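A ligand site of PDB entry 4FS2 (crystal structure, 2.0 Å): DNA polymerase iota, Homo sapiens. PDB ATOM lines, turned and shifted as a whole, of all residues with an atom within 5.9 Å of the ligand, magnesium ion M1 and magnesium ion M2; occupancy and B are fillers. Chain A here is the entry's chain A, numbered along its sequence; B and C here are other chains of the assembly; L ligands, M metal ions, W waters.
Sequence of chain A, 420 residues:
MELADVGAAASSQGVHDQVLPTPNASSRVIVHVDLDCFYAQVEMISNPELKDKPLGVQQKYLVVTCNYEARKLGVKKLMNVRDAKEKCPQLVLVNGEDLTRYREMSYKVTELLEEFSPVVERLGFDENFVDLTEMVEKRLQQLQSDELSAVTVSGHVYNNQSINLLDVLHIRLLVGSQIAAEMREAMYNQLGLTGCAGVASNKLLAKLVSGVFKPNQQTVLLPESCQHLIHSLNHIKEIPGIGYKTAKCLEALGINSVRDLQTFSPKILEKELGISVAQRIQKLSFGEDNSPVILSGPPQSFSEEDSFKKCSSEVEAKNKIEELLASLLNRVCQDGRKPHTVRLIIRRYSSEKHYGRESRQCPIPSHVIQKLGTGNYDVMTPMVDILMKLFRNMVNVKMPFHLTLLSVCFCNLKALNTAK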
ATOM      1  N   HIS A  32      10.544  11.524  33.466  1.00  0.00           N
ATOM      2  CA  HIS A  32      10.471  11.430  31.996  1.00  0.00           C
ATOM      3  C   HIS A  32       9.217  12.145  31.531  1.00  0.00           C
ATOM      4  O   HIS A  32       8.104  11.809  31.989  1.00  0.00           O
ATOM      5  CB  HIS A  32      10.340   9.958  31.607  1.00  0.00           C
ATOM      6  CG  HIS A  32      10.157   9.739  30.136  1.00  0.00           C
ATOM      7  ND1 HIS A  32       8.951   9.299  29.597  1.00  0.00           N
ATOM      8  CD2 HIS A  32      11.015   9.909  29.083  1.00  0.00           C
ATOM      9  CE1 HIS A  32       9.101   9.200  28.254  1.00  0.00           C
ATOM     10  NE2 HIS A  32      10.370   9.572  27.944  1.00  0.00           N
ATOM     11  N   ASP A  34       6.636  13.316  28.330  1.00  0.00           N
ATOM     12  CA  ASP A  34       6.479  12.816  27.011  1.00  0.00           C
ATOM     13  C   ASP A  34       5.230  13.510  26.473  1.00  0.00           C
ATOM     14  O   ASP A  34       4.134  13.253  26.988  1.00  0.00           O
ATOM     15  CB  ASP A  34       6.161  11.312  27.144  1.00  0.00           C
ATOM     16  CG  ASP A  34       5.907  10.662  25.801  1.00  0.00           C
ATOM     17  OD1 ASP A  34       5.488  11.351  24.790  1.00  0.00           O
ATOM     18  OD2 ASP A  34       6.100   9.434  25.755  1.00  0.00           O
ATOM     19  N   LEU A  35       5.373  14.430  25.522  1.00  0.00           N
ATOM     20  CA  LEU A  35       4.183  15.225  25.139  1.00  0.00           C
ATOM     21  C   LEU A  35       3.084  14.400  24.458  1.00  0.00           C
ATOM     22  O   LEU A  35       3.352  13.353  23.849  1.00  0.00           O
ATOM     23  CB  LEU A  35       4.607  16.350  24.216  1.00  0.00           C
ATOM     24  CG  LEU A  35       5.572  17.281  24.966  1.00  0.00           C
ATOM     25  CD1 LEU A  35       5.542  18.600  24.264  1.00  0.00           C
ATOM     26  CD2 LEU A  35       5.160  17.446  26.427  1.00  0.00           C
ATOM     27  N   ASP A  36       1.841  14.890  24.553  1.00  0.00           N
ATOM     28  CA  ASP A  36       0.697  14.196  23.895  1.00  0.00           C
ATOM     29  C   ASP A  36       0.713  14.495  22.358  1.00  0.00           C
ATOM     30  O   ASP A  36       0.879  15.657  21.967  1.00  0.00           O
ATOM     31  CB  ASP A  36      -0.678  14.719  24.436  1.00  0.00           C
ATOM     32  CG  ASP A  36      -0.782  14.591  25.939  1.00  0.00           C
ATOM     33  OD1 ASP A  36      -0.315  13.551  26.480  1.00  0.00           O
ATOM     34  OD2 ASP A  36      -1.382  15.499  26.551  1.00  0.00           O
ATOM     35  N   CYS A  37       0.625  13.429  21.566  1.00  0.00           N
ATOM     36  CA  CYS A  37       0.384  13.470  20.112  1.00  0.00           C
ATOM     37  C   CYS A  37       1.107  14.656  19.438  1.00  0.00           C
ATOM     38  O   CYS A  37       0.526  15.445  18.678  1.00  0.00           O
ATOM     39  CB  CYS A  37      -1.142  13.451  19.817  1.00  0.00           C
ATOM     40  SG  CYS A  37      -2.173  14.789  20.444  1.00  0.00           S
ATOM     41  N   PHE A  38       2.407  14.737  19.726  1.00  0.00           N
ATOM     42  CA  PHE A  38       3.174  15.992  19.552  1.00  0.00           C
ATOM     43  C   PHE A  38       2.931  16.720  18.224  1.00  0.00           C
ATOM     44  O   PHE A  38       2.592  17.889  18.249  1.00  0.00           O
ATOM     45  CB  PHE A  38       4.679  15.737  19.779  1.00  0.00           C
ATOM     46  CG  PHE A  38       5.514  16.988  19.707  1.00  0.00           C
ATOM     47  CD1 PHE A  38       5.234  18.081  20.530  1.00  0.00           C
ATOM     48  CD2 PHE A  38       6.605  17.057  18.827  1.00  0.00           C
ATOM     49  CE1 PHE A  38       6.044  19.257  20.459  1.00  0.00           C
ATOM     50  CE2 PHE A  38       7.410  18.206  18.773  1.00  0.00           C
ATOM     51  CZ  PHE A  38       7.124  19.306  19.576  1.00  0.00           C
ATOM     52  N   TYR A  39       3.143  16.090  17.064  1.00  0.00           N
ATOM     53  CA  TYR A  39       2.961  16.893  15.789  1.00  0.00           C
ATOM     54  C   TYR A  39       1.496  17.423  15.644  1.00  0.00           C
ATOM     55  O   TYR A  39       1.237  18.536  15.137  1.00  0.00           O
ATOM     56  CB  TYR A  39       3.335  16.048  14.583  1.00  0.00           C
ATOM     57  CG  TYR A  39       4.803  15.712  14.392  1.00  0.00           C
ATOM     58  CD1 TYR A  39       5.815  16.040  15.370  1.00  0.00           C
ATOM     59  CD2 TYR A  39       5.186  14.971  13.278  1.00  0.00           C
ATOM     60  CE1 TYR A  39       7.164  15.710  15.147  1.00  0.00           C
ATOM     61  CE2 TYR A  39       6.492  14.641  13.043  1.00  0.00           C
ATOM     62  CZ  TYR A  39       7.482  14.997  13.992  1.00  0.00           C
ATOM     63  OH  TYR A  39       8.750  14.589  13.702  1.00  0.00           O
ATOM     64  N   ALA A  40       0.543  16.625  16.105  1.00  0.00           N
ATOM     65  CA  ALA A  40      -0.885  16.927  15.944  1.00  0.00           C
ATOM     66  C   ALA A  40      -1.225  18.047  16.872  1.00  0.00           C
ATOM     67  O   ALA A  40      -1.942  19.020  16.517  1.00  0.00           O
ATOM     68  CB  ALA A  40      -1.764  15.673  16.214  1.00  0.00           C
ATOM     69  N   GLN A  59       2.780  12.400   6.211  1.00  0.00           N
ATOM     70  CA  GLN A  59       4.025  12.528   5.528  1.00  0.00           C
ATOM     71  C   GLN A  59       3.950  11.511   4.391  1.00  0.00           C
ATOM     72  O   GLN A  59       3.935  10.298   4.668  1.00  0.00           O
ATOM     73  CB  GLN A  59       5.215  12.211   6.480  1.00  0.00           C
ATOM     74  CG  GLN A  59       5.338  13.194   7.625  1.00  0.00           C
ATOM     75  CD  GLN A  59       6.437  12.775   8.622  1.00  0.00           C
ATOM     76  OE1 GLN A  59       6.776  11.597   8.737  1.00  0.00           O
ATOM     77  NE2 GLN A  59       6.992  13.740   9.330  1.00  0.00           N
ATOM     78  N   VAL A  64       1.669   9.733  10.295  1.00  0.00           N
ATOM     79  CA  VAL A  64       2.772   9.548  11.258  1.00  0.00           C
ATOM     80  C   VAL A  64       2.196   9.555  12.662  1.00  0.00           C
ATOM     81  O   VAL A  64       2.457   8.639  13.436  1.00  0.00           O
ATOM     82  CB  VAL A  64       3.959  10.549  11.039  1.00  0.00           C
ATOM     83  CG1 VAL A  64       3.617  12.021  11.397  1.00  0.00           C
ATOM     84  CG2 VAL A  64       5.184  10.064  11.801  1.00  0.00           C
ATOM     85  N   THR A  65       1.334  10.538  12.958  1.00  0.00           N
ATOM     86  CA  THR A  65       0.605  10.520  14.237  1.00  0.00           C
ATOM     87  C   THR A  65      -0.825  11.144  14.094  1.00  0.00           C
ATOM     88  O   THR A  65      -1.130  11.767  13.062  1.00  0.00           O
ATOM     89  CB  THR A  65       1.413  11.251  15.361  1.00  0.00           C
ATOM     90  OG1 THR A  65       0.763  11.026  16.614  1.00  0.00           O
ATOM     91  CG2 THR A  65       1.458  12.784  15.125  1.00  0.00           C
ATOM     92  N   CYS A  66      -1.645  11.058  15.140  1.00  0.00           N
ATOM     93  CA  CYS A  66      -2.985  11.709  15.112  1.00  0.00           C
ATOM     94  C   CYS A  66      -3.394  12.087  16.508  1.00  0.00           C
ATOM     95  O   CYS A  66      -2.847  11.543  17.458  1.00  0.00           O
ATOM     96  CB  CYS A  66      -4.034  10.743  14.560  1.00  0.00           C
ATOM     97  SG  CYS A  66      -3.994   9.191  15.430  1.00  0.00           S
ATOM     98  N   TYR A  68      -6.099  12.564  19.873  1.00  0.00           N
ATOM     99  CA  TYR A  68      -6.808  11.562  20.670  1.00  0.00           C
ATOM    100  C   TYR A  68      -8.261  11.424  20.161  1.00  0.00           C
ATOM    101  O   TYR A  68      -8.819  10.352  20.279  1.00  0.00           O
ATOM    102  CB  TYR A  68      -6.638  11.813  22.209  1.00  0.00           C
ATOM    103  CG  TYR A  68      -5.264  11.288  22.680  1.00  0.00           C
ATOM    104  CD1 TYR A  68      -4.097  12.057  22.457  1.00  0.00           C
ATOM    105  CD2 TYR A  68      -5.113  10.018  23.277  1.00  0.00           C
ATOM    106  CE1 TYR A  68      -2.835  11.581  22.840  1.00  0.00           C
ATOM    107  CE2 TYR A  68      -3.859   9.545  23.664  1.00  0.00           C
ATOM    108  CZ  TYR A  68      -2.717  10.333  23.444  1.00  0.00           C
ATOM    109  OH  TYR A  68      -1.451   9.882  23.756  1.00  0.00           O
ATOM    110  N   ARG A  71      -7.700   8.732  17.628  1.00  0.00           N
ATOM    111  CA  ARG A  71      -7.344   7.390  18.172  1.00  0.00           C
ATOM    112  C   ARG A  71      -8.610   6.710  18.742  1.00  0.00           C
ATOM    113  O   ARG A  71      -8.656   5.496  18.978  1.00  0.00           O
ATOM    114  CB  ARG A  71      -6.248   7.487  19.238  1.00  0.00           C
ATOM    115  CG  ARG A  71      -4.925   8.076  18.732  1.00  0.00           C
ATOM    116  CD  ARG A  71      -3.972   8.397  19.851  1.00  0.00           C
ATOM    117  NE  ARG A  71      -2.833   9.222  19.371  1.00  0.00           N
ATOM    118  CZ  ARG A  71      -1.626   9.184  19.929  1.00  0.00           C
ATOM    119  NH1 ARG A  71      -1.405   8.405  20.971  1.00  0.00           N
ATOM    120  NH2 ARG A  71      -0.620   9.974  19.460  1.00  0.00           N
ATOM    121  N   LYS A  77      -0.920   5.395  15.318  1.00  0.00           N
ATOM    122  CA  LYS A  77       0.303   6.080  14.859  1.00  0.00           C
ATOM    123  C   LYS A  77       0.934   5.202  13.779  1.00  0.00           C
ATOM    124  O   LYS A  77       0.962   3.976  13.897  1.00  0.00           O
ATOM    125  CB  LYS A  77       1.277   6.316  16.036  1.00  0.00           C
ATOM    126  CG  LYS A  77       0.679   7.225  17.103  1.00  0.00           C
ATOM    127  CD  LYS A  77       1.673   7.572  18.205  1.00  0.00           C
ATOM    128  CE  LYS A  77       1.967   6.397  19.096  1.00  0.00           C
ATOM    129  NZ  LYS A  77       2.424   6.872  20.414  1.00  0.00           N
ATOM    130  N   LEU A  78       1.405   5.819  12.714  1.00  0.00           N
ATOM    131  CA  LEU A  78       2.090   5.097  11.637  1.00  0.00           C
ATOM    132  C   LEU A  78       1.172   4.132  10.896  1.00  0.00           C
ATOM    133  O   LEU A  78       1.564   3.021  10.602  1.00  0.00           O
ATOM    134  CB  LEU A  78       3.339   4.369  12.158  1.00  0.00           C
ATOM    135  CG  LEU A  78       4.351   5.189  12.971  1.00  0.00           C
ATOM    136  CD1 LEU A  78       5.080   4.344  14.012  1.00  0.00           C
ATOM    137  CD2 LEU A  78       5.288   5.828  11.956  1.00  0.00           C
ATOM    138  N   PHE A 125      11.907  14.177  19.535  1.00  0.00           N
ATOM    139  CA  PHE A 125      11.494  15.546  19.551  1.00  0.00           C
ATOM    140  C   PHE A 125      10.591  15.819  20.689  1.00  0.00           C
ATOM    141  O   PHE A 125      10.285  16.972  20.938  1.00  0.00           O
ATOM    142  CB  PHE A 125      10.761  15.894  18.244  1.00  0.00           C
ATOM    143  CG  PHE A 125      11.679  16.342  17.102  1.00  0.00           C
ATOM    144  CD1 PHE A 125      13.054  16.043  17.092  1.00  0.00           C
ATOM    145  CD2 PHE A 125      11.145  17.151  16.052  1.00  0.00           C
ATOM    146  CE1 PHE A 125      13.879  16.480  16.021  1.00  0.00           C
ATOM    147  CE2 PHE A 125      11.986  17.601  15.005  1.00  0.00           C
ATOM    148  CZ  PHE A 125      13.332  17.226  14.983  1.00  0.00           C
ATOM    149  N   ASP A 126      10.078  14.790  21.391  1.00  0.00           N
ATOM    150  CA  ASP A 126       9.038  15.123  22.398  1.00  0.00           C
ATOM    151  C   ASP A 126       9.181  14.464  23.748  1.00  0.00           C
ATOM    152  O   ASP A 126       8.235  14.466  24.527  1.00  0.00           O
ATOM    153  CB  ASP A 126       7.619  14.868  21.825  1.00  0.00           C
ATOM    154  CG  ASP A 126       7.107  13.469  22.107  1.00  0.00           C
ATOM    155  OD1 ASP A 126       7.922  12.527  22.034  1.00  0.00           O
ATOM    156  OD2 ASP A 126       5.880  13.322  22.427  1.00  0.00           O
ATOM    157  N   GLU A 127      10.337  13.869  24.027  1.00  0.00           N
ATOM    158  CA  GLU A 127      10.582  13.291  25.381  1.00  0.00           C
ATOM    159  C   GLU A 127      11.852  13.967  25.913  1.00  0.00           C
ATOM    160  O   GLU A 127      12.751  14.270  25.124  1.00  0.00           O
ATOM    161  CB  GLU A 127      10.883  11.822  25.172  1.00  0.00           C
ATOM    162  CG  GLU A 127       9.636  11.105  24.682  1.00  0.00           C
ATOM    163  CD  GLU A 127       9.834   9.592  24.611  1.00  0.00           C
ATOM    164  OE1 GLU A 127      10.671   8.931  25.346  1.00  0.00           O
ATOM    165  OE2 GLU A 127       9.034   9.059  23.875  1.00  0.00           O
ATOM    166  N   LYS A 207      10.492   6.160  32.108  1.00  0.00           N
ATOM    167  CA  LYS A 207       9.920   6.150  30.775  1.00  0.00           C
ATOM    168  C   LYS A 207       8.815   5.066  30.600  1.00  0.00           C
ATOM    169  O   LYS A 207       7.860   5.276  29.882  1.00  0.00           O
ATOM    170  CB  LYS A 207      11.057   5.899  29.759  1.00  0.00           C
ATOM    171  CG  LYS A 207      10.471   5.717  28.342  1.00  0.00           C
ATOM    172  CD  LYS A 207      11.595   5.852  27.279  1.00  0.00           C
ATOM    173  CE  LYS A 207      11.136   5.279  25.929  1.00  0.00           C
ATOM    174  NZ  LYS A 207      10.183   6.248  25.268  1.00  0.00           N
ATOM    175  N   LYS A 214      -2.605   8.088  30.091  1.00  0.00           N
ATOM    176  CA  LYS A 214      -2.487   9.110  29.030  1.00  0.00           C
ATOM    177  C   LYS A 214      -3.880   9.364  28.413  1.00  0.00           C
ATOM    178  O   LYS A 214      -4.731   8.521  28.565  1.00  0.00           O
ATOM    179  CB  LYS A 214      -1.433   8.765  27.986  1.00  0.00           C
ATOM    180  CG  LYS A 214      -1.432   7.361  27.493  1.00  0.00           C
ATOM    181  CD  LYS A 214      -0.064   7.048  26.845  1.00  0.00           C
ATOM    182  CE  LYS A 214       0.041   7.635  25.454  1.00  0.00           C
ATOM    183  NZ  LYS A 214       0.965   6.948  24.496  1.00  0.00           N
ATOM    184  O6  EFG B   4       9.228   5.738  11.937  1.00  0.00           O
ATOM    185  C6  EFG B   4       9.213   5.919  10.750  1.00  0.00           C
ATOM    186  N1  EFG B   4       9.606   4.927   9.933  1.00  0.00           N
ATOM    187  C2  EFG B   4       9.562   5.109   8.574  1.00  0.00           C
ATOM    188  N2  EFG B   4       9.891   4.321   7.606  1.00  0.00           N
ATOM    189  C10 EFG B   4       9.679   4.968   6.487  1.00  0.00           C
ATOM    190  C9  EFG B   4       9.212   6.148   6.777  1.00  0.00           C
ATOM    191  N3  EFG B   4       9.136   6.229   8.064  1.00  0.00           N
ATOM    192  C4  EFG B   4       8.757   7.197   8.858  1.00  0.00           C
ATOM    193  C5  EFG B   4       8.798   7.025  10.173  1.00  0.00           C
ATOM    194  N7  EFG B   4       8.378   8.130  10.702  1.00  0.00           N
ATOM    195  C8  EFG B   4       8.077   8.954   9.727  1.00  0.00           C
ATOM    196  N9  EFG B   4       8.319   8.392   8.587  1.00  0.00           N
ATOM    197  C1' EFG B   4       8.046   9.099   7.295  1.00  0.00           C
ATOM    198  O4' EFG B   4       7.544   8.227   6.335  1.00  0.00           O
ATOM    199  C2' EFG B   4       9.237   9.707   6.609  1.00  0.00           C
ATOM    200  F   EFG B   4      10.216   8.747   6.571  1.00  0.00           F
ATOM    201  C3' EFG B   4       8.824   9.809   5.186  1.00  0.00           C
ATOM    202  O3' EFG B   4       8.399  11.052   4.864  1.00  0.00           O
ATOM    203  C4' EFG B   4       7.563   8.981   5.133  1.00  0.00           C
ATOM    204  C5' EFG B   4       7.572   8.202   3.818  1.00  0.00           C
ATOM    205  O5' EFG B   4       7.838   6.847   3.991  1.00  0.00           O
ATOM    206  P   EFG B   4       8.722   6.033   3.056  1.00  0.00           P
ATOM    207  OP1 EFG B   4       8.241   4.710   3.218  1.00  0.00           O
ATOM    208  OP2 EFG B   4       8.722   6.623   1.750  1.00  0.00           O
ATOM    209  P    DG B   5       9.268  12.119   4.215  1.00  0.00           P
ATOM    210  OP1  DG B   5       8.559  13.270   3.737  1.00  0.00           O
ATOM    211  OP2  DG B   5      10.213  11.454   3.358  1.00  0.00           O
ATOM    212  O5'  DG B   5      10.005  12.620   5.511  1.00  0.00           O
ATOM    213  C5'  DG B   5       9.475  13.668   6.312  1.00  0.00           C
ATOM    214  C4'  DG B   5      10.349  13.866   7.524  1.00  0.00           C
ATOM    215  O4'  DG B   5      10.327  12.662   8.330  1.00  0.00           O
ATOM    216  C3'  DG B   5      11.825  14.153   7.230  1.00  0.00           C
ATOM    217  O3'  DG B   5      12.314  15.288   7.956  1.00  0.00           O
ATOM    218  C2'  DG B   5      12.517  12.875   7.650  1.00  0.00           C
ATOM    219  C1'  DG B   5      11.637  12.457   8.792  1.00  0.00           C
ATOM    220  N9   DG B   5      11.768  11.076   9.225  1.00  0.00           N
ATOM    221  C8   DG B   5      12.071   9.981   8.453  1.00  0.00           C
ATOM    222  N7   DG B   5      12.154   8.878   9.145  1.00  0.00           N
ATOM    223  C5   DG B   5      11.899   9.263  10.449  1.00  0.00           C
ATOM    224  C6   DG B   5      11.847   8.505  11.635  1.00  0.00           C
ATOM    225  O6   DG B   5      12.020   7.294  11.791  1.00  0.00           O
ATOM    226  N1   DG B   5      11.553   9.291  12.735  1.00  0.00           N
ATOM    227  C2   DG B   5      11.313  10.649  12.698  1.00  0.00           C
ATOM    228  N2   DG B   5      11.044  11.227  13.866  1.00  0.00           N
ATOM    229  N3   DG B   5      11.361  11.368  11.598  1.00  0.00           N
ATOM    230  C4   DG B   5      11.661  10.622  10.519  1.00  0.00           C
ATOM    231  N1  DOC C  18      11.338   8.275  17.618  1.00  0.00           N
ATOM    232  C2  DOC C  18      11.354   8.850  16.312  1.00  0.00           C
ATOM    233  N3  DOC C  18      11.546   8.069  15.218  1.00  0.00           N
ATOM    234  C4  DOC C  18      11.739   6.760  15.393  1.00  0.00           C
ATOM    235  C5  DOC C  18      11.711   6.192  16.666  1.00  0.00           C
ATOM    236  C6  DOC C  18      11.525   6.979  17.765  1.00  0.00           C
ATOM    237  O2  DOC C  18      11.212  10.069  16.189  1.00  0.00           O
ATOM    238  N4  DOC C  18      11.964   6.030  14.318  1.00  0.00           N
ATOM    239  C1' DOC C  18      11.153   9.233  18.720  1.00  0.00           C
ATOM    240  C2' DOC C  18       9.678   9.554  18.991  1.00  0.00           C
ATOM    241  C3' DOC C  18       9.352   8.858  20.330  1.00  0.00           C
ATOM    242  C4' DOC C  18      10.744   8.738  20.959  1.00  0.00           C
ATOM    243  O4' DOC C  18      11.725   8.750  19.925  1.00  0.00           O
ATOM    244  C5' DOC C  18      10.919   7.420  21.714  1.00  0.00           C
ATOM    245  O5' DOC C  18      10.875   6.277  20.892  1.00  0.00           O
ATOM    246  P   DOC C  18      11.087   4.819  21.589  1.00  0.00           P
ATOM    247  OP1 DOC C  18      10.399   4.787  22.841  1.00  0.00           O
ATOM    248  OP2 DOC C  18      10.850   3.863  20.509  1.00  0.00           O
HETATM  249  N1  LIG L   1       7.435  10.338  15.176  1.00  0.00           N
HETATM  250  C1  LIG L   1       7.759  10.018  13.874  1.00  0.00           C
HETATM  251  N2  LIG L   1       8.111   8.761  13.625  1.00  0.00           N
HETATM  252  C2  LIG L   1       8.179   7.796  14.560  1.00  0.00           C
HETATM  253  C3  LIG L   1       7.841   8.093  15.829  1.00  0.00           C
HETATM  254  C4  LIG L   1       7.445   9.381  16.106  1.00  0.00           C
HETATM  255  O1  LIG L   1       7.780  10.909  12.953  1.00  0.00           O
HETATM  256  N3  LIG L   1       8.566   6.545  14.195  1.00  0.00           N
HETATM  257  C5  LIG L   1       7.063  11.701  15.506  1.00  0.00           C
HETATM  258  C6  LIG L   1       5.515  11.805  15.533  1.00  0.00           C
HETATM  259  C7  LIG L   1       5.148  12.203  16.972  1.00  0.00           C
HETATM  260  C8  LIG L   1       6.489  12.600  17.644  1.00  0.00           C
HETATM  261  O2  LIG L   1       7.530  12.052  16.847  1.00  0.00           O
HETATM  262  O3  LIG L   1       4.163  13.271  17.038  1.00  0.00           O
HETATM  263  C9  LIG L   1       6.506  12.063  19.091  1.00  0.00           C
HETATM  264  O4  LIG L   1       6.480  10.634  19.097  1.00  0.00           O
HETATM  265  P1  LIG L   1       5.664   9.789  20.206  1.00  0.00           P
HETATM  266  O5  LIG L   1       5.767  10.525  21.548  1.00  0.00           O
HETATM  267  O6  LIG L   1       5.844   8.349  20.014  1.00  0.00           O
HETATM  268  O7  LIG L   1       4.134   9.974  19.625  1.00  0.00           O
HETATM  269  P2  LIG L   1       3.034  11.121  19.937  1.00  0.00           P
HETATM  270  O8  LIG L   1       2.485  11.616  18.584  1.00  0.00           O
HETATM  271  O9  LIG L   1       3.664  12.212  20.808  1.00  0.00           O
HETATM  272  O10 LIG L   1       1.832  10.344  20.701  1.00  0.00           O
HETATM  273  P3  LIG L   1       1.772   9.976  22.271  1.00  0.00           P
HETATM  274  O11 LIG L   1       3.154  10.291  22.831  1.00  0.00           O
HETATM  275  O12 LIG L   1       0.690  10.911  22.717  1.00  0.00           O
HETATM  276  O13 LIG L   1       1.453   8.466  22.172  1.00  0.00           O
HETATM  277 MG    MG M   1       4.622  11.793  22.795  1.00  0.00          MG
HETATM  278 MG    MG M   2       7.148   9.850  22.994  1.00  0.00          MG
HETATM  279  O   HOH W   1       8.952  12.903  11.623  1.00  0.00           O
HETATM  280  O   HOH W   2       2.485  11.007  25.863  1.00  0.00           O
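DOC 18 of chain C touches magnesium ion M2. Within 4 Å of magnesium ion M2: Asp 34, Asp 126, Glu 127 and DOC 18 of chain C.
Three residues have an atom within 4 Å of magnesium ion M1: Asp 34, Leu 35 and Asp 126. Along chain A the residues within 4 Å of magnesium ion M1 span positions 34 to 126. The nearest printed residue that does not touch magnesium ion M1 is Cys 37 (4.5 Å).
The side-chain amino group of Lys 207 is in salt-bridge range of the side-chain carboxylate of Glu 127 (2.7 Å). The side-chain carboxylate (OE1) of Glu 127 lies within hydrogen-bond range of a ring nitrogen (NE2) of His 32. NH1 of Arg 71 is in hydrogen-bond range of OH of Tyr 68. NH2 of Arg 71 is in hydrogen-bond range of OG1 of Thr 65, 3.3 Å away. NE of Arg 71 is in hydrogen-bond range of O of Cys 66. The backbone NH (N) of Leu 78 is in hydrogen-bond range of the backbone carbonyl oxygen (O) of Val 64 (3.1 Å). N2 of DG 5 of chain B lies close to O2 of DOC 18 of chain C (2.6 Å). The side-chain amino group of Lys 207 is in salt-bridge range of OP1 of DOC 18 of chain C (2.8 Å).
An oxygen (O1) of the ligand sits close to N2 of DG 5 of chain B, 3.4 Å away. CA of Asp 36 touches O12 of the ligand (3.5 Å). Val 64 touches the ligand (CG2 to O1, 3.0 Å). Hydrophobic or aromatic side chains within 4 Å of the ligand: Phe 38, Tyr 39, Val 64 and Tyr 68. 16 residues have an atom within 4 Å of the ligand: Asp 34, Leu 35, Asp 36, Cys 37, Phe 38, Tyr 39, Val 64, Thr 65, Tyr 68, Arg 71, Lys 77, Asp 126, Lys 214, EFG 4 of chain B, DG 5 of chain B and DOC 18 of chain C. The nearest printed residue that does not touch the ligand is Leu 78 (4.03 Å).
Magnesium ion M1 is bound by OD2 of Asp 126, O11 of the ligand, O5 of the ligand, OD1 of Asp 34, O9 of the ligand and O of Leu 35. Magnesium ion M1 has six donor atoms within binding distance.
Water W1 lies within hydrogen-bond range of an oxygen (O1) of the ligand (2.7 Å), the side-chain hydroxyl (OH) of Tyr 39 (2.7 Å), N3 of DG 5 of chain B (2.9 Å) and the side-chain amide nitrogen (NE2) of Gln 59 (3.1 Å).
O6 of EFG 4 of chain B sits at hydrogen-bond distance from N3 of the ligand (2.5 Å). The side-chain amino group (NZ) of Lys 77 is in salt-bridge range of an oxygen (O13) of the ligand (2.6 Å). An oxygen (O12) of the ligand is in hydrogen-bond range of the side-chain hydroxyl of Tyr 68. OG1 of Thr 65 is in hydrogen-bond range of O8 of the ligand, at 2.7 Å. N of Cys 37 is in hydrogen-bond range of O12 of the ligand (2.8 Å). NH1 of Arg 71 is in salt-bridge range of O13 of the ligand (3.1 Å). The side-chain amino group of Lys 214 is in salt-bridge range of an oxygen (O13) of the ligand (2.8 Å). N of Tyr 39 sits at hydrogen-bond distance from O3 of the ligand. The backbone NH (N) of Phe 38 lies within hydrogen-bond range of an oxygen (O8) of the ligand, 3.3 Å away. A nitrogen (N3) of the ligand sits close to N4 of DOC 18 of chain C, 3.4 Å away.
Magnesium ion M2 is bound by an oxygen (O5) of the ligand (2.1 Å) and the side-chain carboxylate (OE2) of Glu 127 (2.2 Å). Magnesium ion M2 has two donor atoms within binding distance.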
